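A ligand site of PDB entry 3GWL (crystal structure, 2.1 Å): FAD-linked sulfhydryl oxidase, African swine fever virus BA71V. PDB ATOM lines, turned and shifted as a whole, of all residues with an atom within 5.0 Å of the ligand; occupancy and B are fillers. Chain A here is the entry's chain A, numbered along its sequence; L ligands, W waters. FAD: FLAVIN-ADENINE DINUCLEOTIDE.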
ATOM      1  N   MET A   4      19.070  18.284  25.558  1.00  0.00           N
ATOM      2  CA  MET A   4      17.650  18.474  25.255  1.00  0.00           C
ATOM      3  C   MET A   4      17.028  19.823  25.627  1.00  0.00           C
ATOM      4  O   MET A   4      15.960  20.152  25.119  1.00  0.00           O
ATOM      5  CB  MET A   4      16.835  17.333  25.844  1.00  0.00           C
ATOM      6  CG  MET A   4      17.060  16.003  25.118  1.00  0.00           C
ATOM      7  SD  MET A   4      16.784  16.103  23.329  1.00  0.00           S
ATOM      8  CE  MET A   4      15.002  15.895  23.235  1.00  0.00           C
ATOM      9  N   LEU A   5      17.671  20.607  26.495  1.00  0.00           N
ATOM     10  CA  LEU A   5      17.107  21.909  26.841  1.00  0.00           C
ATOM     11  C   LEU A   5      17.160  22.812  25.611  1.00  0.00           C
ATOM     12  O   LEU A   5      16.434  23.804  25.514  1.00  0.00           O
ATOM     13  CB  LEU A   5      17.893  22.572  27.973  1.00  0.00           C
ATOM     14  CG  LEU A   5      17.789  22.003  29.400  1.00  0.00           C
ATOM     15  CD1 LEU A   5      18.469  23.004  30.339  1.00  0.00           C
ATOM     16  CD2 LEU A   5      16.329  21.772  29.806  1.00  0.00           C
ATOM     17  N   GLY A   8      15.171  19.977  22.559  1.00  0.00           N
ATOM     18  CA  GLY A   8      13.809  19.621  22.904  1.00  0.00           C
ATOM     19  C   GLY A   8      12.729  20.513  22.296  1.00  0.00           C
ATOM     20  O   GLY A   8      11.824  20.012  21.625  1.00  0.00           O
ATOM     21  N   PRO A   9      12.806  21.830  22.516  1.00  0.00           N
ATOM     22  CA  PRO A   9      11.815  22.771  21.969  1.00  0.00           C
ATOM     23  C   PRO A   9      11.663  22.686  20.455  1.00  0.00           C
ATOM     24  O   PRO A   9      10.558  22.803  19.934  1.00  0.00           O
ATOM     25  CB  PRO A   9      12.345  24.130  22.435  1.00  0.00           C
ATOM     26  CG  PRO A   9      13.032  23.798  23.736  1.00  0.00           C
ATOM     27  CD  PRO A   9      13.770  22.527  23.375  1.00  0.00           C
ATOM     28  N   TYR A  11      12.019  20.078  18.528  1.00  0.00           N
ATOM     29  CA  TYR A  11      11.235  18.895  18.183  1.00  0.00           C
ATOM     30  C   TYR A  11       9.755  19.062  18.528  1.00  0.00           C
ATOM     31  O   TYR A  11       8.883  18.634  17.763  1.00  0.00           O
ATOM     32  CB  TYR A  11      11.806  17.637  18.846  1.00  0.00           C
ATOM     33  CG  TYR A  11      13.073  17.158  18.186  1.00  0.00           C
ATOM     34  CD1 TYR A  11      14.311  17.724  18.497  1.00  0.00           C
ATOM     35  CD2 TYR A  11      13.032  16.198  17.180  1.00  0.00           C
ATOM     36  CE1 TYR A  11      15.475  17.347  17.806  1.00  0.00           C
ATOM     37  CE2 TYR A  11      14.175  15.815  16.494  1.00  0.00           C
ATOM     38  CZ  TYR A  11      15.402  16.390  16.808  1.00  0.00           C
ATOM     39  OH  TYR A  11      16.530  16.033  16.088  1.00  0.00           O
ATOM     40  N   TRP A  12       9.456  19.660  19.673  1.00  0.00           N
ATOM     41  CA  TRP A  12       8.060  19.872  20.043  1.00  0.00           C
ATOM     42  C   TRP A  12       7.396  20.788  19.021  1.00  0.00           C
ATOM     43  O   TRP A  12       6.245  20.562  18.636  1.00  0.00           O
ATOM     44  CB  TRP A  12       7.949  20.493  21.443  1.00  0.00           C
ATOM     45  CG  TRP A  12       8.215  19.526  22.550  1.00  0.00           C
ATOM     46  CD1 TRP A  12       9.198  19.615  23.486  1.00  0.00           C
ATOM     47  CD2 TRP A  12       7.513  18.304  22.808  1.00  0.00           C
ATOM     48  NE1 TRP A  12       9.150  18.523  24.325  1.00  0.00           N
ATOM     49  CE2 TRP A  12       8.124  17.703  23.927  1.00  0.00           C
ATOM     50  CE3 TRP A  12       6.420  17.664  22.209  1.00  0.00           C
ATOM     51  CZ2 TRP A  12       7.688  16.483  24.462  1.00  0.00           C
ATOM     52  CZ3 TRP A  12       5.986  16.448  22.736  1.00  0.00           C
ATOM     53  CH2 TRP A  12       6.626  15.875  23.850  1.00  0.00           C
ATOM     54  N   HIS A  16       3.983  19.853  16.937  1.00  0.00           N
ATOM     55  CA  HIS A  16       2.741  20.622  17.013  1.00  0.00           C
ATOM     56  C   HIS A  16       2.353  21.292  15.702  1.00  0.00           C
ATOM     57  O   HIS A  16       1.171  21.391  15.399  1.00  0.00           O
ATOM     58  CB  HIS A  16       2.841  21.675  18.120  1.00  0.00           C
ATOM     59  CG  HIS A  16       3.045  21.068  19.482  1.00  0.00           C
ATOM     60  ND1 HIS A  16       2.180  20.130  20.009  1.00  0.00           N
ATOM     61  CD2 HIS A  16       4.003  21.259  20.410  1.00  0.00           C
ATOM     62  CE1 HIS A  16       2.614  19.762  21.198  1.00  0.00           C
ATOM     63  NE2 HIS A  16       3.722  20.433  21.464  1.00  0.00           N
ATOM     64  N   PHE A  41       9.358  10.703  13.384  1.00  0.00           N
ATOM     65  CA  PHE A  41       9.638  11.786  14.318  1.00  0.00           C
ATOM     66  C   PHE A  41      10.283  11.219  15.583  1.00  0.00           C
ATOM     67  O   PHE A  41      11.275  11.769  16.088  1.00  0.00           O
ATOM     68  CB  PHE A  41       8.350  12.523  14.677  1.00  0.00           C
ATOM     69  CG  PHE A  41       8.487  13.466  15.835  1.00  0.00           C
ATOM     70  CD1 PHE A  41       9.092  14.710  15.664  1.00  0.00           C
ATOM     71  CD2 PHE A  41       8.015  13.110  17.091  1.00  0.00           C
ATOM     72  CE1 PHE A  41       9.226  15.589  16.745  1.00  0.00           C
ATOM     73  CE2 PHE A  41       8.138  13.985  18.178  1.00  0.00           C
ATOM     74  CZ  PHE A  41       8.753  15.229  18.009  1.00  0.00           C
ATOM     75  N   LEU A  45      14.476  11.544  17.390  1.00  0.00           N
ATOM     76  CA  LEU A  45      14.820  12.099  18.709  1.00  0.00           C
ATOM     77  C   LEU A  45      16.271  11.754  19.061  1.00  0.00           C
ATOM     78  O   LEU A  45      16.689  10.611  18.923  1.00  0.00           O
ATOM     79  CB  LEU A  45      13.872  11.557  19.778  1.00  0.00           C
ATOM     80  CG  LEU A  45      12.418  12.024  19.702  1.00  0.00           C
ATOM     81  CD1 LEU A  45      11.555  11.204  20.652  1.00  0.00           C
ATOM     82  CD2 LEU A  45      12.344  13.513  20.033  1.00  0.00           C
ATOM     83  N   ARG A  49      16.397   7.136  25.620  1.00  0.00           N
ATOM     84  CA  ARG A  49      15.340   7.152  26.619  1.00  0.00           C
ATOM     85  C   ARG A  49      14.116   7.912  26.126  1.00  0.00           C
ATOM     86  O   ARG A  49      12.982   7.510  26.401  1.00  0.00           O
ATOM     87  CB  ARG A  49      15.857   7.788  27.913  1.00  0.00           C
ATOM     88  CG  ARG A  49      15.338   9.191  28.203  1.00  0.00           C
ATOM     89  CD  ARG A  49      16.012   9.772  29.425  1.00  0.00           C
ATOM     90  NE  ARG A  49      17.424  10.062  29.157  1.00  0.00           N
ATOM     91  CZ  ARG A  49      17.889  11.267  28.866  1.00  0.00           C
ATOM     92  NH1 ARG A  49      17.063  12.304  28.811  1.00  0.00           N
ATOM     93  NH2 ARG A  49      19.173  11.440  28.620  1.00  0.00           N
ATOM     94  N   CYS A  50      14.341   8.995  25.376  1.00  0.00           N
ATOM     95  CA  CYS A  50      13.242   9.801  24.847  1.00  0.00           C
ATOM     96  C   CYS A  50      12.432   9.013  23.828  1.00  0.00           C
ATOM     97  O   CYS A  50      11.210   9.129  23.754  1.00  0.00           O
ATOM     98  CB  CYS A  50      13.787  11.072  24.194  1.00  0.00           C
ATOM     99  SG  CYS A  50      14.896  12.055  25.243  1.00  0.00           S
ATOM    100  N   HIS A  53      10.227   6.260  25.667  1.00  0.00           N
ATOM    101  CA  HIS A  53       9.074   6.834  26.347  1.00  0.00           C
ATOM    102  C   HIS A  53       8.017   7.170  25.301  1.00  0.00           C
ATOM    103  O   HIS A  53       6.853   6.820  25.439  1.00  0.00           O
ATOM    104  CB  HIS A  53       9.465   8.093  27.115  1.00  0.00           C
ATOM    105  CG  HIS A  53      10.239   7.833  28.363  1.00  0.00           C
ATOM    106  ND1 HIS A  53       9.688   7.186  29.459  1.00  0.00           N
ATOM    107  CD2 HIS A  53      11.515   8.128  28.711  1.00  0.00           C
ATOM    108  CE1 HIS A  53      10.604   7.098  30.419  1.00  0.00           C
ATOM    109  NE2 HIS A  53      11.717   7.655  29.982  1.00  0.00           N
ATOM    110  N   ALA A  54       8.438   7.860  24.242  1.00  0.00           N
ATOM    111  CA  ALA A  54       7.522   8.266  23.184  1.00  0.00           C
ATOM    112  C   ALA A  54       6.860   7.034  22.560  1.00  0.00           C
ATOM    113  O   ALA A  54       5.649   7.020  22.342  1.00  0.00           O
ATOM    114  CB  ALA A  54       8.265   9.048  22.118  1.00  0.00           C
ATOM    115  N   THR A  75      -1.056  15.688  20.314  1.00  0.00           N
ATOM    116  CA  THR A  75       0.323  16.145  20.544  1.00  0.00           C
ATOM    117  C   THR A  75       0.424  16.947  21.841  1.00  0.00           C
ATOM    118  O   THR A  75       1.402  16.848  22.567  1.00  0.00           O
ATOM    119  CB  THR A  75       0.859  17.001  19.361  1.00  0.00           C
ATOM    120  OG1 THR A  75       0.137  18.231  19.284  1.00  0.00           O
ATOM    121  CG2 THR A  75       0.720  16.255  18.031  1.00  0.00           C
ATOM    122  N   PHE A  76      -0.609  17.751  22.112  1.00  0.00           N
ATOM    123  CA  PHE A  76      -0.696  18.561  23.318  1.00  0.00           C
ATOM    124  C   PHE A  76      -0.674  17.675  24.578  1.00  0.00           C
ATOM    125  O   PHE A  76       0.085  17.946  25.518  1.00  0.00           O
ATOM    126  CB  PHE A  76      -2.000  19.372  23.270  1.00  0.00           C
ATOM    127  CG  PHE A  76      -2.459  19.904  24.596  1.00  0.00           C
ATOM    128  CD1 PHE A  76      -1.843  21.007  25.171  1.00  0.00           C
ATOM    129  CD2 PHE A  76      -3.528  19.323  25.253  1.00  0.00           C
ATOM    130  CE1 PHE A  76      -2.302  21.530  26.379  1.00  0.00           C
ATOM    131  CE2 PHE A  76      -3.997  19.831  26.464  1.00  0.00           C
ATOM    132  CZ  PHE A  76      -3.379  20.953  27.026  1.00  0.00           C
ATOM    133  N   PHE A  78       0.349  14.558  24.765  1.00  0.00           N
ATOM    134  CA  PHE A  78       1.612  13.830  24.792  1.00  0.00           C
ATOM    135  C   PHE A  78       2.684  14.747  25.372  1.00  0.00           C
ATOM    136  O   PHE A  78       3.519  14.323  26.194  1.00  0.00           O
ATOM    137  CB  PHE A  78       2.010  13.389  23.379  1.00  0.00           C
ATOM    138  CG  PHE A  78       3.398  12.819  23.279  1.00  0.00           C
ATOM    139  CD1 PHE A  78       3.894  11.957  24.258  1.00  0.00           C
ATOM    140  CD2 PHE A  78       4.210  13.117  22.191  1.00  0.00           C
ATOM    141  CE1 PHE A  78       5.160  11.408  24.151  1.00  0.00           C
ATOM    142  CE2 PHE A  78       5.480  12.568  22.061  1.00  0.00           C
ATOM    143  CZ  PHE A  78       5.955  11.700  23.046  1.00  0.00           C
ATOM    144  N   HIS A  79       2.662  15.998  24.943  1.00  0.00           N
ATOM    145  CA  HIS A  79       3.636  16.973  25.425  1.00  0.00           C
ATOM    146  C   HIS A  79       3.477  17.171  26.941  1.00  0.00           C
ATOM    147  O   HIS A  79       4.467  17.234  27.661  1.00  0.00           O
ATOM    148  CB  HIS A  79       3.472  18.291  24.682  1.00  0.00           C
ATOM    149  CG  HIS A  79       4.622  19.238  24.857  1.00  0.00           C
ATOM    150  ND1 HIS A  79       4.956  20.201  23.926  1.00  0.00           N
ATOM    151  CD2 HIS A  79       5.506  19.385  25.877  1.00  0.00           C
ATOM    152  CE1 HIS A  79       5.982  20.900  24.365  1.00  0.00           C
ATOM    153  NE2 HIS A  79       6.342  20.426  25.545  1.00  0.00           N
ATOM    154  N   ASN A  80       2.232  17.261  27.417  1.00  0.00           N
ATOM    155  CA  ASN A  80       2.017  17.426  28.851  1.00  0.00           C
ATOM    156  C   ASN A  80       2.421  16.191  29.650  1.00  0.00           C
ATOM    157  O   ASN A  80       2.782  16.290  30.828  1.00  0.00           O
ATOM    158  CB  ASN A  80       0.556  17.764  29.151  1.00  0.00           C
ATOM    159  CG  ASN A  80       0.305  19.256  29.152  1.00  0.00           C
ATOM    160  OD1 ASN A  80       1.201  20.046  29.437  1.00  0.00           O
ATOM    161  ND2 ASN A  80      -0.923  19.639  28.852  1.00  0.00           N
ATOM    162  N   VAL A  82       4.997  14.350  28.994  1.00  0.00           N
ATOM    163  CA  VAL A  82       6.442  14.465  29.184  1.00  0.00           C
ATOM    164  C   VAL A  82       6.705  15.580  30.210  1.00  0.00           C
ATOM    165  O   VAL A  82       7.603  15.459  31.049  1.00  0.00           O
ATOM    166  CB  VAL A  82       7.180  14.799  27.865  1.00  0.00           C
ATOM    167  CG1 VAL A  82       8.624  15.165  28.160  1.00  0.00           C
ATOM    168  CG2 VAL A  82       7.150  13.594  26.928  1.00  0.00           C
ATOM    169  N   ASN A  83       5.916  16.654  30.158  1.00  0.00           N
ATOM    170  CA  ASN A  83       6.098  17.737  31.134  1.00  0.00           C
ATOM    171  C   ASN A  83       5.937  17.147  32.542  1.00  0.00           C
ATOM    172  O   ASN A  83       6.711  17.450  33.443  1.00  0.00           O
ATOM    173  CB  ASN A  83       5.077  18.857  30.946  1.00  0.00           C
ATOM    174  CG  ASN A  83       5.355  19.723  29.719  1.00  0.00           C
ATOM    175  OD1 ASN A  83       6.469  19.746  29.203  1.00  0.00           O
ATOM    176  ND2 ASN A  83       4.339  20.448  29.262  1.00  0.00           N
ATOM    177  N   ARG A  85       6.322  13.978  33.503  1.00  0.00           N
ATOM    178  CA  ARG A  85       7.413  13.063  33.818  1.00  0.00           C
ATOM    179  C   ARG A  85       8.672  13.810  34.247  1.00  0.00           C
ATOM    180  O   ARG A  85       9.499  13.273  34.976  1.00  0.00           O
ATOM    181  CB  ARG A  85       7.726  12.152  32.628  1.00  0.00           C
ATOM    182  CG  ARG A  85       8.830  11.158  32.949  1.00  0.00           C
ATOM    183  CD  ARG A  85       9.018  10.075  31.891  1.00  0.00           C
ATOM    184  NE  ARG A  85       9.728  10.546  30.695  1.00  0.00           N
ATOM    185  CZ  ARG A  85       9.132  11.067  29.629  1.00  0.00           C
ATOM    186  NH1 ARG A  85       7.811  11.183  29.597  1.00  0.00           N
ATOM    187  NH2 ARG A  85       9.850  11.463  28.588  1.00  0.00           N
ATOM    188  N   LEU A  86       8.807  15.060  33.796  1.00  0.00           N
ATOM    189  CA  LEU A  86       9.977  15.873  34.133  1.00  0.00           C
ATOM    190  C   LEU A  86       9.605  16.884  35.218  1.00  0.00           C
ATOM    191  O   LEU A  86      10.369  17.793  35.522  1.00  0.00           O
ATOM    192  CB  LEU A  86      10.474  16.647  32.902  1.00  0.00           C
ATOM    193  CG  LEU A  86      10.909  15.836  31.679  1.00  0.00           C
ATOM    194  CD1 LEU A  86      11.352  16.778  30.594  1.00  0.00           C
ATOM    195  CD2 LEU A  86      12.030  14.892  32.062  1.00  0.00           C
ATOM    196  N   LYS A  88       7.523  19.275  35.140  1.00  0.00           N
ATOM    197  CA  LYS A  88       7.451  20.613  34.567  1.00  0.00           C
ATOM    198  C   LYS A  88       5.975  21.039  34.570  1.00  0.00           C
ATOM    199  O   LYS A  88       5.100  20.220  34.828  1.00  0.00           O
ATOM    200  CB  LYS A  88       7.983  20.617  33.129  1.00  0.00           C
ATOM    201  CG  LYS A  88       9.454  20.271  33.008  1.00  0.00           C
ATOM    202  CD  LYS A  88       9.861  19.996  31.557  1.00  0.00           C
ATOM    203  CE  LYS A  88       9.722  21.231  30.695  1.00  0.00           C
ATOM    204  NZ  LYS A  88      10.588  22.352  31.168  1.00  0.00           N
ATOM    205  N   LYS A  89       5.716  22.301  34.282  1.00  0.00           N
ATOM    206  CA  LYS A  89       4.341  22.795  34.266  1.00  0.00           C
ATOM    207  C   LYS A  89       3.450  22.136  33.211  1.00  0.00           C
ATOM    208  O   LYS A  89       3.881  21.885  32.081  1.00  0.00           O
ATOM    209  CB  LYS A  89       4.320  24.311  34.053  1.00  0.00           C
ATOM    210  CG  LYS A  89       2.916  24.902  34.060  1.00  0.00           C
ATOM    211  CD  LYS A  89       2.900  26.386  33.706  1.00  0.00           C
ATOM    212  CE  LYS A  89       1.464  26.863  33.525  1.00  0.00           C
ATOM    213  NZ  LYS A  89       1.377  28.267  33.018  1.00  0.00           N
ATOM    214  N   ILE A  91       0.524  22.883  31.038  1.00  0.00           N
ATOM    215  CA  ILE A  91      -0.272  23.991  30.548  1.00  0.00           C
ATOM    216  C   ILE A  91      -1.688  23.586  30.157  1.00  0.00           C
ATOM    217  O   ILE A  91      -1.957  22.411  29.892  1.00  0.00           O
ATOM    218  CB  ILE A  91       0.389  24.692  29.327  1.00  0.00           C
ATOM    219  CG1 ILE A  91       0.284  23.823  28.074  1.00  0.00           C
ATOM    220  CG2 ILE A  91       1.842  25.014  29.646  1.00  0.00           C
ATOM    221  CD1 ILE A  91       0.692  24.555  26.787  1.00  0.00           C
ATOM    222  N   TYR A  96      -2.342  26.544  25.277  1.00  0.00           N
ATOM    223  CA  TYR A  96      -1.771  25.951  24.084  1.00  0.00           C
ATOM    224  C   TYR A  96      -2.266  26.754  22.882  1.00  0.00           C
ATOM    225  O   TYR A  96      -1.489  27.158  22.024  1.00  0.00           O
ATOM    226  CB  TYR A  96      -2.228  24.490  23.938  1.00  0.00           C
ATOM    227  CG  TYR A  96      -2.160  24.013  22.505  1.00  0.00           C
ATOM    228  CD1 TYR A  96      -0.944  23.697  21.909  1.00  0.00           C
ATOM    229  CD2 TYR A  96      -3.321  23.937  21.719  1.00  0.00           C
ATOM    230  CE1 TYR A  96      -0.874  23.329  20.553  1.00  0.00           C
ATOM    231  CE2 TYR A  96      -3.263  23.577  20.366  1.00  0.00           C
ATOM    232  CZ  TYR A  96      -2.030  23.276  19.791  1.00  0.00           C
ATOM    233  OH  TYR A  96      -1.956  22.944  18.455  1.00  0.00           O
ATOM    234  N   ILE A  99      -0.596  30.036  22.583  1.00  0.00           N
ATOM    235  CA  ILE A  99       0.786  29.873  22.157  1.00  0.00           C
ATOM    236  C   ILE A  99       0.926  29.633  20.651  1.00  0.00           C
ATOM    237  O   ILE A  99       1.827  30.196  20.028  1.00  0.00           O
ATOM    238  CB  ILE A  99       1.449  28.696  22.909  1.00  0.00           C
ATOM    239  CG1 ILE A  99       1.654  29.079  24.380  1.00  0.00           C
ATOM    240  CG2 ILE A  99       2.768  28.340  22.263  1.00  0.00           C
ATOM    241  CD1 ILE A  99       2.099  27.918  25.268  1.00  0.00           C
ATOM    242  N   TYR A 100       0.039  28.824  20.085  1.00  0.00           N
ATOM    243  CA  TYR A 100       0.109  28.518  18.648  1.00  0.00           C
ATOM    244  C   TYR A 100      -0.968  29.194  17.795  1.00  0.00           C
ATOM    245  O   TYR A 100      -1.144  28.836  16.624  1.00  0.00           O
ATOM    246  CB  TYR A 100       0.031  27.004  18.441  1.00  0.00           C
ATOM    247  CG  TYR A 100       1.331  26.284  18.715  1.00  0.00           C
ATOM    248  CD1 TYR A 100       1.621  25.752  19.969  1.00  0.00           C
ATOM    249  CD2 TYR A 100       2.300  26.186  17.720  1.00  0.00           C
ATOM    250  CE1 TYR A 100       2.859  25.136  20.220  1.00  0.00           C
ATOM    251  CE2 TYR A 100       3.519  25.583  17.962  1.00  0.00           C
ATOM    252  CZ  TYR A 100       3.799  25.064  19.210  1.00  0.00           C
ATOM    253  OH  TYR A 100       5.018  24.469  19.389  1.00  0.00           O
HETATM  254  PA  FAD L   1       9.416  22.376  26.106  1.00  0.00           P
HETATM  255  O1A FAD L   1       8.652  21.337  26.845  1.00  0.00           O
HETATM  256  O2A FAD L   1      10.668  22.272  25.296  1.00  0.00           O
HETATM  257  O5B FAD L   1       8.658  23.571  25.429  1.00  0.00           O
HETATM  258  C5B FAD L   1       8.165  23.886  24.125  1.00  0.00           C
HETATM  259  C4B FAD L   1       7.345  25.081  24.571  1.00  0.00           C
HETATM  260  O4B FAD L   1       6.021  24.698  24.115  1.00  0.00           O
HETATM  261  C3B FAD L   1       7.032  25.930  25.842  1.00  0.00           C
HETATM  262  O3B FAD L   1       8.070  26.813  26.275  1.00  0.00           O
HETATM  263  C2B FAD L   1       5.651  26.405  25.748  1.00  0.00           C
HETATM  264  O2B FAD L   1       5.658  27.486  24.852  1.00  0.00           O
HETATM  265  C1B FAD L   1       5.036  25.206  25.023  1.00  0.00           C
HETATM  266  N9A FAD L   1       4.439  24.067  25.645  1.00  0.00           N
HETATM  267  C8A FAD L   1       4.533  23.472  26.929  1.00  0.00           C
HETATM  268  N7A FAD L   1       3.760  22.475  27.236  1.00  0.00           N
HETATM  269  C5A FAD L   1       3.072  22.270  26.045  1.00  0.00           C
HETATM  270  C6A FAD L   1       2.051  21.428  25.557  1.00  0.00           C
HETATM  271  N6A FAD L   1       1.500  20.480  26.328  1.00  0.00           N
HETATM  272  N1A FAD L   1       1.635  21.505  24.233  1.00  0.00           N
HETATM  273  C2A FAD L   1       2.124  22.369  23.319  1.00  0.00           C
HETATM  274  N3A FAD L   1       3.113  23.232  23.802  1.00  0.00           N
HETATM  275  C4A FAD L   1       3.513  23.145  25.164  1.00  0.00           C
HETATM  276  N1  FAD L   1      13.948  15.536  28.107  1.00  0.00           N
HETATM  277  C2  FAD L   1      14.487  14.806  29.148  1.00  0.00           C
HETATM  278  O2  FAD L   1      15.363  15.261  29.882  1.00  0.00           O
HETATM  279  N3  FAD L   1      14.046  13.485  29.157  1.00  0.00           N
HETATM  280  C4  FAD L   1      13.137  12.943  28.226  1.00  0.00           C
HETATM  281  O4  FAD L   1      12.834  11.718  28.349  1.00  0.00           O
HETATM  282  C4X FAD L   1      12.641  13.746  27.206  1.00  0.00           C
HETATM  283  N5  FAD L   1      11.718  13.261  26.223  1.00  0.00           N
HETATM  284  C5X FAD L   1      11.253  13.981  25.108  1.00  0.00           C
HETATM  285  C6  FAD L   1      10.384  13.324  24.215  1.00  0.00           C
HETATM  286  C7  FAD L   1       9.954  14.051  23.074  1.00  0.00           C
HETATM  287  C7M FAD L   1       9.021  13.238  22.183  1.00  0.00           C
HETATM  288  C8  FAD L   1      10.425  15.363  22.772  1.00  0.00           C
HETATM  289  C8M FAD L   1      10.113  16.279  21.597  1.00  0.00           C
HETATM  290  C9  FAD L   1      11.290  15.953  23.709  1.00  0.00           C
HETATM  291  C9A FAD L   1      11.732  15.375  24.916  1.00  0.00           C
HETATM  292  N10 FAD L   1      12.592  15.800  26.051  1.00  0.00           N
HETATM  293  C10 FAD L   1      13.106  15.091  27.111  1.00  0.00           C
HETATM  294  C1' FAD L   1      12.795  17.212  26.156  1.00  0.00           C
HETATM  295  C2' FAD L   1      11.871  18.090  26.946  1.00  0.00           C
HETATM  296  O2' FAD L   1      10.489  17.700  26.716  1.00  0.00           O
HETATM  297  C3' FAD L   1      11.966  19.581  26.771  1.00  0.00           C
HETATM  298  O3' FAD L   1      11.884  19.890  25.388  1.00  0.00           O
HETATM  299  C4' FAD L   1      13.110  20.305  27.466  1.00  0.00           C
HETATM  300  O4' FAD L   1      13.409  19.850  28.817  1.00  0.00           O
HETATM  301  C5' FAD L   1      13.108  21.773  27.446  1.00  0.00           C
HETATM  302  O5' FAD L   1      12.008  22.315  28.185  1.00  0.00           O
HETATM  303  P   FAD L   1      11.320  23.694  27.929  1.00  0.00           P
HETATM  304  O1P FAD L   1      11.152  24.169  29.291  1.00  0.00           O
HETATM  305  O2P FAD L   1      12.031  24.560  26.958  1.00  0.00           O
HETATM  306  O3P FAD L   1       9.908  23.444  27.177  1.00  0.00           O
HETATM  307  O   HOH W   1      14.686  25.099  26.782  1.00  0.00           O
HETATM  308  O   HOH W   2       6.053  23.647  21.533  1.00  0.00           O
HETATM  309  O   HOH W   3       7.042  22.484  28.884  1.00  0.00           O
HETATM  310  O   HOH W   4       8.788  24.655  21.041  1.00  0.00           O
HETATM  311  O   HOH W   5      15.560  17.873  28.664  1.00  0.00           O
HETATM  312  O   HOH W   6      13.042  21.572  30.900  1.00  0.00           O
HETATM  313  O   HOH W   7      11.496  26.941  25.571  1.00  0.00           O
HETATM  314  O   HOH W   8       8.749  19.014  28.220  1.00  0.00           O
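The backbone NH (N) of Lys 88 sits at hydrogen-bond distance from the backbone carbonyl oxygen (O) of Asn 83 (2.6 Å). A ring nitrogen (ND1) of His 79 lies within hydrogen-bond range of a ring nitrogen (NE2) of His 16 (2.8 Å). The side-chain amide nitrogen (ND2) of Asn 83 sits at hydrogen-bond distance from the side-chain amide oxygen (OD1) of Asn 80. The backbone carbonyl oxygen (O) of Lys 89 sits at hydrogen-bond distance from the side-chain amide nitrogen (ND2) of Asn 83 (3.2 Å). A ring nitrogen (ND1) of His 16 lies within hydrogen-bond range of the side-chain hydroxyl (OG1) of Thr 75, at 2.9 Å. The backbone carbonyl oxygen (O) of Ile 91 lies within hydrogen-bond range of the side-chain amide nitrogen (ND2) of Asn 80, 3.1 Å away.
A nitrogen (N3) of the ligand sits close to the guanidinium group (NH1) of Arg 49, 3.3 Å away. The side-chain sulfur (SG) of Cys 50 lies close to a nitrogen (N5) of the ligand, 3.5 Å away. Met 4 touches the ligand. Leu 5 touches the ligand. Gly 8 touches the ligand (CA to O3', 3.2 Å). CG of Pro 9 touches O2A of the ligand, at 3.2 Å. CB of Tyr 11 touches C8M of the ligand, at 3.5 Å. NE2 of His 16 touches C2A of the ligand, at 3.1 Å. Phe 41 touches the ligand. Leu 45 touches the ligand (CD1 to C7M, 3.6 Å). CD2 of His 53 touches O4 of the ligand, at 3.8 Å. Phe 78 touches the ligand. Val 82 touches the ligand (CG1 to O2', 3.5 Å). Leu 86 touches the ligand (CD1 to N1, 3.8 Å). CD1 of Ile 91 touches C5A of the ligand (3.4 Å). Tyr 96 touches the ligand. Ile 99 touches the ligand. Hydrophobic or aromatic side chains within 4 Å of the ligand: Met 4, Leu 5, Pro 9, Tyr 11, Trp 12, His 16, Phe 41, Leu 45, His 53, Phe 76, Phe 78, His 79, Val 82, Leu 86, Ile 91, Tyr 96 and Ile 99. 24 residues have an atom within 4 Å of the ligand: Met 4, Leu 5, Gly 8, Pro 9, Tyr 11, Trp 12, His 16, Phe 41, Leu 45, Arg 49, Cys 50, His 53, Phe 76, Phe 78, His 79, Asn 80, Val 82, Asn 83, Arg 85, Leu 86, Lys 88, Ile 91, Tyr 96 and Ile 99.
Water W8 bridges the side-chain amide oxygen of Asn 83 (2.6 Å) and an oxygen (O2') of the ligand (2.6 Å). Water W1 lies within hydrogen-bond range of the backbone carbonyl oxygen of Leu 5 (2.5 Å) and an oxygen (O2P) of the ligand (2.7 Å). Water W6 lies within hydrogen-bond range of NZ of Lys 88 (2.6 Å) and O4' of the ligand (2.7 Å). Water W2 bridges the side-chain hydroxyl (OH) of Tyr 100 and an oxygen (O4B) of the ligand. Water W3 bridges the side-chain amide oxygen (OD1) of Asn 83 (2.8 Å) and an oxygen (O1A) of the ligand (2.8 Å).
An oxygen (O1P) of the ligand is in salt-bridge range of the side-chain amino group of Lys 88 (2.7 Å). An oxygen (O1A) of the ligand lies within hydrogen-bond range of a ring nitrogen (NE2) of His 79 (2.8 Å). The indole nitrogen (NE1) of Trp 12 sits at hydrogen-bond distance from an oxygen (O2') of the ligand. ND2 of Asn 83 is in hydrogen-bond range of N7A of the ligand, 2.9 Å away. The guanidinium group (NH2) of Arg 85 lies within hydrogen-bond range of an oxygen (O4) of the ligand (3.0 Å). N6A of the ligand sits at hydrogen-bond distance from O of Phe 76, 3.0 Å away. OD1 of Asn 80 lies within hydrogen-bond range of N6A of the ligand, at 3.2 Å.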
